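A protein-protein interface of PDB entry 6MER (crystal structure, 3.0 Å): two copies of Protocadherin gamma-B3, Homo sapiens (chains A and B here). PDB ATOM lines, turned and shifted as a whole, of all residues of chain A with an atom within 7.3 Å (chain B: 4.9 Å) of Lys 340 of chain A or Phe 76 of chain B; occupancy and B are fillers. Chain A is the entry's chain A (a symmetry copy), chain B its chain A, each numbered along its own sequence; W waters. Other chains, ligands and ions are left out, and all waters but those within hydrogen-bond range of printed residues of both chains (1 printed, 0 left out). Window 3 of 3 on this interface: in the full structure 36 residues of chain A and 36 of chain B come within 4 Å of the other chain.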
ATOM      1  N   GLU A 316      16.104  36.981 -10.812  1.00  0.00           N
ATOM      2  CA  GLU A 316      15.445  35.744 -10.428  1.00  0.00           C
ATOM      3  C   GLU A 316      16.252  35.036  -9.346  1.00  0.00           C
ATOM      4  O   GLU A 316      17.479  35.151  -9.280  1.00  0.00           O
ATOM      5  CB  GLU A 316      15.252  34.823 -11.635  1.00  0.00           C
ATOM      6  CG  GLU A 316      16.517  34.150 -12.140  1.00  0.00           C
ATOM      7  CD  GLU A 316      16.244  33.209 -13.297  1.00  0.00           C
ATOM      8  OE1 GLU A 316      15.444  33.573 -14.184  1.00  0.00           O
ATOM      9  OE2 GLU A 316      16.820  32.100 -13.315  1.00  0.00           O
ATOM     10  N   ILE A 317      15.545  34.306  -8.488  1.00  0.00           N
ATOM     11  CA  ILE A 317      16.133  33.662  -7.320  1.00  0.00           C
ATOM     12  C   ILE A 317      16.044  32.153  -7.499  1.00  0.00           C
ATOM     13  O   ILE A 317      14.964  31.614  -7.771  1.00  0.00           O
ATOM     14  CB  ILE A 317      15.430  34.103  -6.024  1.00  0.00           C
ATOM     15  CG1 ILE A 317      15.490  35.625  -5.883  1.00  0.00           C
ATOM     16  CG2 ILE A 317      16.063  33.426  -4.819  1.00  0.00           C
ATOM     17  CD1 ILE A 317      14.766  36.150  -4.666  1.00  0.00           C
ATOM     18  N   THR A 318      17.179  31.476  -7.346  1.00  0.00           N
ATOM     19  CA  THR A 318      17.255  30.023  -7.408  1.00  0.00           C
ATOM     20  C   THR A 318      17.593  29.488  -6.023  1.00  0.00           C
ATOM     21  O   THR A 318      18.577  29.917  -5.412  1.00  0.00           O
ATOM     22  CB  THR A 318      18.305  29.567  -8.424  1.00  0.00           C
ATOM     23  OG1 THR A 318      17.969  30.073  -9.722  1.00  0.00           O
ATOM     24  CG2 THR A 318      18.368  28.048  -8.478  1.00  0.00           C
ATOM     25  N   LEU A 319      16.778  28.558  -5.533  1.00  0.00           N
ATOM     26  CA  LEU A 319      16.928  28.019  -4.191  1.00  0.00           C
ATOM     27  C   LEU A 319      17.267  26.535  -4.248  1.00  0.00           C
ATOM     28  O   LEU A 319      16.975  25.843  -5.228  1.00  0.00           O
ATOM     29  CB  LEU A 319      15.655  28.233  -3.363  1.00  0.00           C
ATOM     30  CG  LEU A 319      15.222  29.689  -3.173  1.00  0.00           C
ATOM     31  CD1 LEU A 319      13.943  29.768  -2.355  1.00  0.00           C
ATOM     32  CD2 LEU A 319      16.331  30.497  -2.517  1.00  0.00           C
ATOM     33  N   ALA A 320      17.890  26.055  -3.175  1.00  0.00           N
ATOM     34  CA  ALA A 320      18.255  24.653  -3.050  1.00  0.00           C
ATOM     35  C   ALA A 320      18.433  24.331  -1.574  1.00  0.00           C
ATOM     36  O   ALA A 320      18.928  25.162  -0.810  1.00  0.00           O
ATOM     37  CB  ALA A 320      19.537  24.331  -3.827  1.00  0.00           C
ATOM     38  N   LEU A 338      20.480  27.180   0.033  1.00  0.00           N
ATOM     39  CA  LEU A 338      21.440  27.839  -0.838  1.00  0.00           C
ATOM     40  C   LEU A 338      20.705  28.761  -1.801  1.00  0.00           C
ATOM     41  O   LEU A 338      19.686  28.379  -2.385  1.00  0.00           O
ATOM     42  CB  LEU A 338      22.269  26.817  -1.620  1.00  0.00           C
ATOM     43  CG  LEU A 338      23.121  25.863  -0.781  1.00  0.00           C
ATOM     44  CD1 LEU A 338      23.903  24.916  -1.675  1.00  0.00           C
ATOM     45  CD2 LEU A 338      24.054  26.644   0.132  1.00  0.00           C
ATOM     46  N   ILE A 339      21.228  29.973  -1.967  1.00  0.00           N
ATOM     47  CA  ILE A 339      20.598  31.007  -2.778  1.00  0.00           C
ATOM     48  C   ILE A 339      21.551  31.397  -3.897  1.00  0.00           C
ATOM     49  O   ILE A 339      22.730  31.678  -3.646  1.00  0.00           O
ATOM     50  CB  ILE A 339      20.218  32.237  -1.933  1.00  0.00           C
ATOM     51  CG1 ILE A 339      19.297  31.831  -0.782  1.00  0.00           C
ATOM     52  CG2 ILE A 339      19.557  33.299  -2.799  1.00  0.00           C
ATOM     53  CD1 ILE A 339      18.878  32.984   0.097  1.00  0.00           C
ATOM     54  N   LYS A 340      21.043  31.413  -5.128  1.00  0.00           N
ATOM     55  CA  LYS A 340      21.788  31.895  -6.283  1.00  0.00           C
ATOM     56  C   LYS A 340      20.967  32.962  -6.985  1.00  0.00           C
ATOM     57  O   LYS A 340      19.787  32.746  -7.283  1.00  0.00           O
ATOM     58  CB  LYS A 340      22.122  30.762  -7.258  1.00  0.00           C
ATOM     59  CG  LYS A 340      22.871  31.234  -8.496  1.00  0.00           C
ATOM     60  CD  LYS A 340      23.049  30.114  -9.508  1.00  0.00           C
ATOM     61  CE  LYS A 340      23.823  30.594 -10.726  1.00  0.00           C
ATOM     62  NZ  LYS A 340      24.050  29.501 -11.711  1.00  0.00           N
ATOM     63  N   THR A 341      21.587  34.109  -7.245  1.00  0.00           N
ATOM     64  CA  THR A 341      20.934  35.221  -7.915  1.00  0.00           C
ATOM     65  C   THR A 341      21.727  35.616  -9.152  1.00  0.00           C
ATOM     66  O   THR A 341      22.955  35.504  -9.183  1.00  0.00           O
ATOM     67  CB  THR A 341      20.796  36.436  -6.986  1.00  0.00           C
ATOM     68  OG1 THR A 341      22.096  36.963  -6.689  1.00  0.00           O
ATOM     69  CG2 THR A 341      20.106  36.045  -5.688  1.00  0.00           C
ATOM     70  N   HIS A 342      21.013  36.076 -10.176  1.00  0.00           N
ATOM     71  CA  HIS A 342      21.655  36.610 -11.367  1.00  0.00           C
ATOM     72  C   HIS A 342      20.654  37.485 -12.105  1.00  0.00           C
ATOM     73  O   HIS A 342      19.463  37.171 -12.153  1.00  0.00           O
ATOM     74  CB  HIS A 342      22.177  35.497 -12.285  1.00  0.00           C
ATOM     75  CG  HIS A 342      21.098  34.704 -12.953  1.00  0.00           C
ATOM     76  ND1 HIS A 342      20.610  33.525 -12.432  1.00  0.00           N
ATOM     77  CD2 HIS A 342      20.418  34.916 -14.105  1.00  0.00           C
ATOM     78  CE1 HIS A 342      19.673  33.047 -13.231  1.00  0.00           C
ATOM     79  NE2 HIS A 342      19.537  33.873 -14.253  1.00  0.00           N
ATOM     80  N   ILE A 352      22.892  42.818  -7.634  1.00  0.00           N
ATOM     81  CA  ILE A 352      21.734  42.383  -6.866  1.00  0.00           C
ATOM     82  C   ILE A 352      22.040  42.510  -5.381  1.00  0.00           C
ATOM     83  O   ILE A 352      23.158  42.225  -4.940  1.00  0.00           O
ATOM     84  CB  ILE A 352      21.343  40.935  -7.221  1.00  0.00           C
ATOM     85  CG1 ILE A 352      21.161  40.792  -8.731  1.00  0.00           C
ATOM     86  CG2 ILE A 352      20.073  40.522  -6.495  1.00  0.00           C
ATOM     87  CD1 ILE A 352      20.864  39.386  -9.174  1.00  0.00           C
ATOM     88  N   ASN A 370      27.091  36.345  -6.205  1.00  0.00           N
ATOM     89  CA  ASN A 370      25.811  35.822  -6.654  1.00  0.00           C
ATOM     90  C   ASN A 370      25.309  34.628  -5.853  1.00  0.00           C
ATOM     91  O   ASN A 370      24.193  34.164  -6.108  1.00  0.00           O
ATOM     92  CB  ASN A 370      25.891  35.430  -8.137  1.00  0.00           C
ATOM     93  CG  ASN A 370      25.931  36.635  -9.058  1.00  0.00           C
ATOM     94  OD1 ASN A 370      25.380  37.690  -8.743  1.00  0.00           O
ATOM     95  ND2 ASN A 370      26.582  36.482 -10.206  1.00  0.00           N
ATOM     96  N   THR A 371      26.086  34.121  -4.900  1.00  0.00           N
ATOM     97  CA  THR A 371      25.703  32.955  -4.114  1.00  0.00           C
ATOM     98  C   THR A 371      25.581  33.344  -2.648  1.00  0.00           C
ATOM     99  O   THR A 371      26.512  33.918  -2.075  1.00  0.00           O
ATOM    100  CB  THR A 371      26.719  31.819  -4.270  1.00  0.00           C
ATOM    101  OG1 THR A 371      28.002  32.255  -3.803  1.00  0.00           O
ATOM    102  CG2 THR A 371      26.830  31.400  -5.728  1.00  0.00           C
ATOM    103  N   TYR A 372      24.435  33.029  -2.052  1.00  0.00           N
ATOM    104  CA  TYR A 372      24.178  33.284  -0.644  1.00  0.00           C
ATOM    105  C   TYR A 372      23.864  31.973   0.064  1.00  0.00           C
ATOM    106  O   TYR A 372      23.467  30.984  -0.558  1.00  0.00           O
ATOM    107  CB  TYR A 372      23.020  34.273  -0.456  1.00  0.00           C
ATOM    108  CG  TYR A 372      23.279  35.642  -1.043  1.00  0.00           C
ATOM    109  CD1 TYR A 372      23.818  36.660  -0.268  1.00  0.00           C
ATOM    110  CD2 TYR A 372      22.984  35.916  -2.371  1.00  0.00           C
ATOM    111  CE1 TYR A 372      24.056  37.914  -0.800  1.00  0.00           C
ATOM    112  CE2 TYR A 372      23.219  37.167  -2.913  1.00  0.00           C
ATOM    113  CZ  TYR A 372      23.756  38.161  -2.122  1.00  0.00           C
ATOM    114  OH  TYR A 372      23.991  39.408  -2.656  1.00  0.00           O
ATOM    115  N   ARG A 373      24.043  31.975   1.383  1.00  0.00           N
ATOM    116  CA  ARG A 373      23.824  30.792   2.202  1.00  0.00           C
ATOM    117  C   ARG A 373      22.946  31.161   3.389  1.00  0.00           C
ATOM    118  O   ARG A 373      23.267  32.091   4.136  1.00  0.00           O
ATOM    119  CB  ARG A 373      25.154  30.200   2.683  1.00  0.00           C
ATOM    120  CG  ARG A 373      25.045  28.786   3.228  1.00  0.00           C
ATOM    121  CD  ARG A 373      26.415  28.189   3.529  1.00  0.00           C
ATOM    122  NE  ARG A 373      27.023  28.757   4.730  1.00  0.00           N
ATOM    123  CZ  ARG A 373      27.947  29.713   4.724  1.00  0.00           C
ATOM    124  NH1 ARG A 373      28.442  30.165   5.868  1.00  0.00           N
ATOM    125  NH2 ARG A 373      28.376  30.218   3.575  1.00  0.00           N
ATOM    126  N   ALA A 394      15.157  39.693  -3.621  1.00  0.00           N
ATOM    127  CA  ALA A 394      16.379  40.173  -4.253  1.00  0.00           C
ATOM    128  C   ALA A 394      16.036  41.369  -5.127  1.00  0.00           C
ATOM    129  O   ALA A 394      15.198  41.261  -6.029  1.00  0.00           O
ATOM    130  CB  ALA A 394      17.041  39.070  -5.080  1.00  0.00           C
ATOM    131  N   VAL B  38      22.575  19.433 -10.154  1.00  0.00           N
ATOM    132  CA  VAL B  38      22.955  20.558 -11.001  1.00  0.00           C
ATOM    133  C   VAL B  38      21.715  21.418 -11.196  1.00  0.00           C
ATOM    134  O   VAL B  38      20.738  20.975 -11.813  1.00  0.00           O
ATOM    135  CB  VAL B  38      23.524  20.103 -12.353  1.00  0.00           C
ATOM    136  CG1 VAL B  38      23.548  21.262 -13.337  1.00  0.00           C
ATOM    137  CG2 VAL B  38      24.921  19.538 -12.171  1.00  0.00           C
ATOM    138  N   ILE B  39      21.746  22.637 -10.669  1.00  0.00           N
ATOM    139  CA  ILE B  39      20.656  23.591 -10.831  1.00  0.00           C
ATOM    140  C   ILE B  39      20.996  24.507 -12.000  1.00  0.00           C
ATOM    141  O   ILE B  39      22.066  25.127 -12.026  1.00  0.00           O
ATOM    142  CB  ILE B  39      20.405  24.394  -9.545  1.00  0.00           C
ATOM    143  CG1 ILE B  39      21.722  24.907  -8.954  1.00  0.00           C
ATOM    144  CG2 ILE B  39      19.655  23.548  -8.528  1.00  0.00           C
ATOM    145  CD1 ILE B  39      21.533  25.865  -7.799  1.00  0.00           C
ATOM    146  N   ALA B  40      20.092  24.581 -12.972  1.00  0.00           N
ATOM    147  CA  ALA B  40      20.298  25.409 -14.149  1.00  0.00           C
ATOM    148  C   ALA B  40      18.953  25.664 -14.810  1.00  0.00           C
ATOM    149  O   ALA B  40      18.123  24.757 -14.908  1.00  0.00           O
ATOM    150  CB  ALA B  40      21.262  24.747 -15.141  1.00  0.00           C
ATOM    151  N   PHE B  45      23.220  19.707 -18.646  1.00  0.00           N
ATOM    152  CA  PHE B  45      24.111  18.722 -18.053  1.00  0.00           C
ATOM    153  C   PHE B  45      23.437  18.061 -16.860  1.00  0.00           C
ATOM    154  O   PHE B  45      22.549  18.639 -16.227  1.00  0.00           O
ATOM    155  CB  PHE B  45      25.435  19.355 -17.606  1.00  0.00           C
ATOM    156  CG  PHE B  45      26.179  20.049 -18.709  1.00  0.00           C
ATOM    157  CD1 PHE B  45      26.035  21.412 -18.909  1.00  0.00           C
ATOM    158  CD2 PHE B  45      27.024  19.340 -19.547  1.00  0.00           C
ATOM    159  CE1 PHE B  45      26.719  22.054 -19.923  1.00  0.00           C
ATOM    160  CE2 PHE B  45      27.710  19.976 -20.563  1.00  0.00           C
ATOM    161  CZ  PHE B  45      27.557  21.335 -20.750  1.00  0.00           C
ATOM    162  N   LEU B  54      30.052  14.179 -14.566  1.00  0.00           N
ATOM    163  CA  LEU B  54      29.240  15.198 -15.217  1.00  0.00           C
ATOM    164  C   LEU B  54      29.032  14.805 -16.675  1.00  0.00           C
ATOM    165  O   LEU B  54      29.998  14.703 -17.439  1.00  0.00           O
ATOM    166  CB  LEU B  54      29.906  16.570 -15.115  1.00  0.00           C
ATOM    167  CG  LEU B  54      29.190  17.734 -15.803  1.00  0.00           C
ATOM    168  CD1 LEU B  54      27.812  17.950 -15.202  1.00  0.00           C
ATOM    169  CD2 LEU B  54      30.020  19.005 -15.714  1.00  0.00           C
ATOM    170  N   LEU B  74      29.507  28.102 -20.432  1.00  0.00           N
ATOM    171  CA  LEU B  74      28.298  27.919 -19.642  1.00  0.00           C
ATOM    172  C   LEU B  74      28.685  27.814 -18.175  1.00  0.00           C
ATOM    173  O   LEU B  74      29.538  26.998 -17.812  1.00  0.00           O
ATOM    174  CB  LEU B  74      27.528  26.671 -20.082  1.00  0.00           C
ATOM    175  CG  LEU B  74      26.892  26.728 -21.472  1.00  0.00           C
ATOM    176  CD1 LEU B  74      26.098  25.461 -21.754  1.00  0.00           C
ATOM    177  CD2 LEU B  74      26.008  27.957 -21.600  1.00  0.00           C
ATOM    178  N   GLU B  75      28.060  28.640 -17.339  1.00  0.00           N
ATOM    179  CA  GLU B  75      28.372  28.708 -15.916  1.00  0.00           C
ATOM    180  C   GLU B  75      27.131  28.316 -15.125  1.00  0.00           C
ATOM    181  O   GLU B  75      26.129  29.039 -15.135  1.00  0.00           O
ATOM    182  CB  GLU B  75      28.852  30.106 -15.529  1.00  0.00           C
ATOM    183  CG  GLU B  75      30.075  30.576 -16.300  1.00  0.00           C
ATOM    184  CD  GLU B  75      30.536  31.958 -15.880  1.00  0.00           C
ATOM    185  OE1 GLU B  75      30.008  32.484 -14.877  1.00  0.00           O
ATOM    186  OE2 GLU B  75      31.426  32.520 -16.554  1.00  0.00           O
ATOM    187  N   PHE B  76      27.199  27.174 -14.446  1.00  0.00           N
ATOM    188  CA  PHE B  76      26.134  26.713 -13.570  1.00  0.00           C
ATOM    189  C   PHE B  76      26.720  26.385 -12.204  1.00  0.00           C
ATOM    190  O   PHE B  76      27.939  26.396 -12.005  1.00  0.00           O
ATOM    191  CB  PHE B  76      25.404  25.494 -14.156  1.00  0.00           C
ATOM    192  CG  PHE B  76      26.287  24.295 -14.364  1.00  0.00           C
ATOM    193  CD1 PHE B  76      26.415  23.331 -13.377  1.00  0.00           C
ATOM    194  CD2 PHE B  76      26.981  24.126 -15.552  1.00  0.00           C
ATOM    195  CE1 PHE B  76      27.224  22.226 -13.566  1.00  0.00           C
ATOM    196  CE2 PHE B  76      27.791  23.023 -15.748  1.00  0.00           C
ATOM    197  CZ  PHE B  76      27.911  22.071 -14.754  1.00  0.00           C
ATOM    198  N   GLU B  77      25.838  26.090 -11.255  1.00  0.00           N
ATOM    199  CA  GLU B  77      26.227  25.790  -9.886  1.00  0.00           C
ATOM    200  C   GLU B  77      25.869  24.350  -9.546  1.00  0.00           C
ATOM    201  O   GLU B  77      24.818  23.847  -9.955  1.00  0.00           O
ATOM    202  CB  GLU B  77      25.550  26.744  -8.895  1.00  0.00           C
ATOM    203  CG  GLU B  77      26.034  28.184  -8.983  1.00  0.00           C
ATOM    204  CD  GLU B  77      27.406  28.384  -8.368  1.00  0.00           C
ATOM    205  OE1 GLU B  77      27.890  27.466  -7.673  1.00  0.00           O
ATOM    206  OE2 GLU B  77      27.999  29.463  -8.575  1.00  0.00           O
ATOM    207  N   MET B  78      26.751  23.695  -8.798  1.00  0.00           N
ATOM    208  CA  MET B  78      26.540  22.336  -8.325  1.00  0.00           C
ATOM    209  C   MET B  78      26.209  22.368  -6.839  1.00  0.00           C
ATOM    210  O   MET B  78      26.851  23.089  -6.067  1.00  0.00           O
ATOM    211  CB  MET B  78      27.778  21.472  -8.571  1.00  0.00           C
ATOM    212  CG  MET B  78      27.542  19.984  -8.393  1.00  0.00           C
ATOM    213  SD  MET B  78      29.063  19.034  -8.568  1.00  0.00           S
ATOM    214  CE  MET B  78      28.406  17.387  -8.807  1.00  0.00           C
ATOM    215  N   PHE B  86      28.019  25.297  -2.458  1.00  0.00           N
ATOM    216  CA  PHE B  86      27.926  25.590  -3.879  1.00  0.00           C
ATOM    217  C   PHE B  86      29.260  25.311  -4.557  1.00  0.00           C
ATOM    218  O   PHE B  86      30.324  25.545  -3.977  1.00  0.00           O
ATOM    219  CB  PHE B  86      27.516  27.046  -4.113  1.00  0.00           C
ATOM    220  CG  PHE B  86      26.051  27.229  -4.388  1.00  0.00           C
ATOM    221  CD1 PHE B  86      25.304  26.205  -4.944  1.00  0.00           C
ATOM    222  CD2 PHE B  86      25.422  28.427  -4.094  1.00  0.00           C
ATOM    223  CE1 PHE B  86      23.956  26.371  -5.200  1.00  0.00           C
ATOM    224  CE2 PHE B  86      24.074  28.599  -4.347  1.00  0.00           C
ATOM    225  CZ  PHE B  86      23.340  27.570  -4.903  1.00  0.00           C
ATOM    226  N   PHE B  87      29.195  24.810  -5.788  1.00  0.00           N
ATOM    227  CA  PHE B  87      30.382  24.509  -6.587  1.00  0.00           C
ATOM    228  C   PHE B  87      30.157  25.061  -7.992  1.00  0.00           C
ATOM    229  O   PHE B  87      29.426  24.468  -8.789  1.00  0.00           O
ATOM    230  CB  PHE B  87      30.664  23.009  -6.616  1.00  0.00           C
ATOM    231  CG  PHE B  87      31.013  22.434  -5.272  1.00  0.00           C
ATOM    232  CD1 PHE B  87      32.319  22.463  -4.809  1.00  0.00           C
ATOM    233  CD2 PHE B  87      30.036  21.864  -4.472  1.00  0.00           C
ATOM    234  CE1 PHE B  87      32.642  21.935  -3.574  1.00  0.00           C
ATOM    235  CE2 PHE B  87      30.354  21.336  -3.236  1.00  0.00           C
ATOM    236  CZ  PHE B  87      31.660  21.370  -2.787  1.00  0.00           C
ATOM    237  N   HIS B  88      30.786  26.196  -8.288  1.00  0.00           N
ATOM    238  CA  HIS B  88      30.630  26.826  -9.593  1.00  0.00           C
ATOM    239  C   HIS B  88      31.415  26.048 -10.641  1.00  0.00           C
ATOM    240  O   HIS B  88      32.634  25.886 -10.522  1.00  0.00           O
ATOM    241  CB  HIS B  88      31.097  28.278  -9.538  1.00  0.00           C
ATOM    242  CG  HIS B  88      30.808  29.054 -10.785  1.00  0.00           C
ATOM    243  ND1 HIS B  88      31.637  29.029 -11.885  1.00  0.00           N
ATOM    244  CD2 HIS B  88      29.781  29.875 -11.106  1.00  0.00           C
ATOM    245  CE1 HIS B  88      31.134  29.803 -12.831  1.00  0.00           C
ATOM    246  NE2 HIS B  88      30.007  30.328 -12.383  1.00  0.00           N
ATOM    247  N   VAL B  89      30.718  25.565 -11.665  1.00  0.00           N
ATOM    248  CA  VAL B  89      31.317  24.774 -12.733  1.00  0.00           C
ATOM    249  C   VAL B  89      31.156  25.540 -14.037  1.00  0.00           C
ATOM    250  O   VAL B  89      30.033  25.882 -14.429  1.00  0.00           O
ATOM    251  CB  VAL B  89      30.680  23.379 -12.837  1.00  0.00           C
ATOM    252  CG1 VAL B  89      31.375  22.559 -13.914  1.00  0.00           C
ATOM    253  CG2 VAL B  89      30.737  22.668 -11.494  1.00  0.00           C
ATOM    254  N   VAL B  91      31.783  25.479 -18.171  1.00  0.00           N
ATOM    255  CA  VAL B  91      31.923  24.548 -19.285  1.00  0.00           C
ATOM    256  C   VAL B  91      32.070  25.364 -20.561  1.00  0.00           C
ATOM    257  O   VAL B  91      31.108  25.998 -21.012  1.00  0.00           O
ATOM    258  CB  VAL B  91      30.737  23.580 -19.393  1.00  0.00           C
ATOM    259  CG1 VAL B  91      30.912  22.668 -20.597  1.00  0.00           C
ATOM    260  CG2 VAL B  91      30.601  22.762 -18.118  1.00  0.00           C
HETATM  261  O   HOH W   1      23.115  30.353 -14.585  1.00  0.00           O
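O of Glu 77 of chain B is in hydrogen-bond range of N of Ile 39 of chain B (3.4 Å).
The backbone carbonyl oxygen of Phe 76 of chain B is in hydrogen-bond range of the backbone NH of Val 89 of chain B (2.9 Å).
The backbone NH (N) of His 88 of chain B lies within hydrogen-bond range of the side-chain carboxylate (OE1) of Glu 77 of chain B, 3.2 Å away.
O of Thr 318 of chain A lies within hydrogen-bond range of N of Lys 340 of chain A, 2.9 Å away.
The backbone NH of Leu 338 of chain A sits at hydrogen-bond distance from the backbone carbonyl oxygen of Ala 320 of chain A (2.7 Å).
O of Ile 339 of chain A lies within hydrogen-bond range of N of Tyr 372 of chain A (2.7 Å).
Thr 318 of chain A touches Ile 39 of chain B.
CB of Leu 338 of chain A touches CZ of Phe 86 of chain B, 3.5 Å away.
Phe 86 of chain B touches Ile 339 of chain A (CE2 to O, 3.4 Å).
Lys 340 of chain A touches Phe 76 of chain B (NZ to CA, 3.9 Å).
Glu 77 of chain B touches Lys 340 of chain A (CG to CD, 3.6 Å).
OE2 of Glu 77 of chain B touches CG2 of Thr 371 of chain A (3.6 Å).
Thr 371 of chain A touches Phe 86 of chain B.
Lys 340 of chain A touches two residues of chain B.
Phe 76 of chain B touches just one residue of chain A: Lys 340 (3.9 Å).
Printed residues of chain A within 4 Å of Glu 77 of chain B: Lys 340 (3.6 Å) and Thr 371 (3.6 Å).
Of the printed residues of chain B, Thr 371 of chain A touches Glu 77 and Phe 86.
Of the printed residues of chain A, Ile 39 of chain B touches Thr 318.
His 342 of chain A touches none of the printed residues of chain B.
The nearest residue of chain B that does not touch Lys 340 of chain A is Glu 75 of chain B (4.03 Å).
Hydrophobic or aromatic side chains of chain A that line the printed part of chain B: Leu 338.
Printed residues of chain B that touch a printed residue of chain A: Ile 39, Phe 76, Glu 77 and Phe 86.
Among the printed residues, 7 pairs touch across the chains.
Among the printed residues, no Asp or Glu carboxylate lies within 4 Å of a Lys or Arg side-chain nitrogen of the other chain.
No position is printed for both chains.
Water W1 lies within hydrogen-bond range of NZ of Lys 340 of chain A (3.1 Å) and O of Glu 75 of chain B (3.3 Å).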
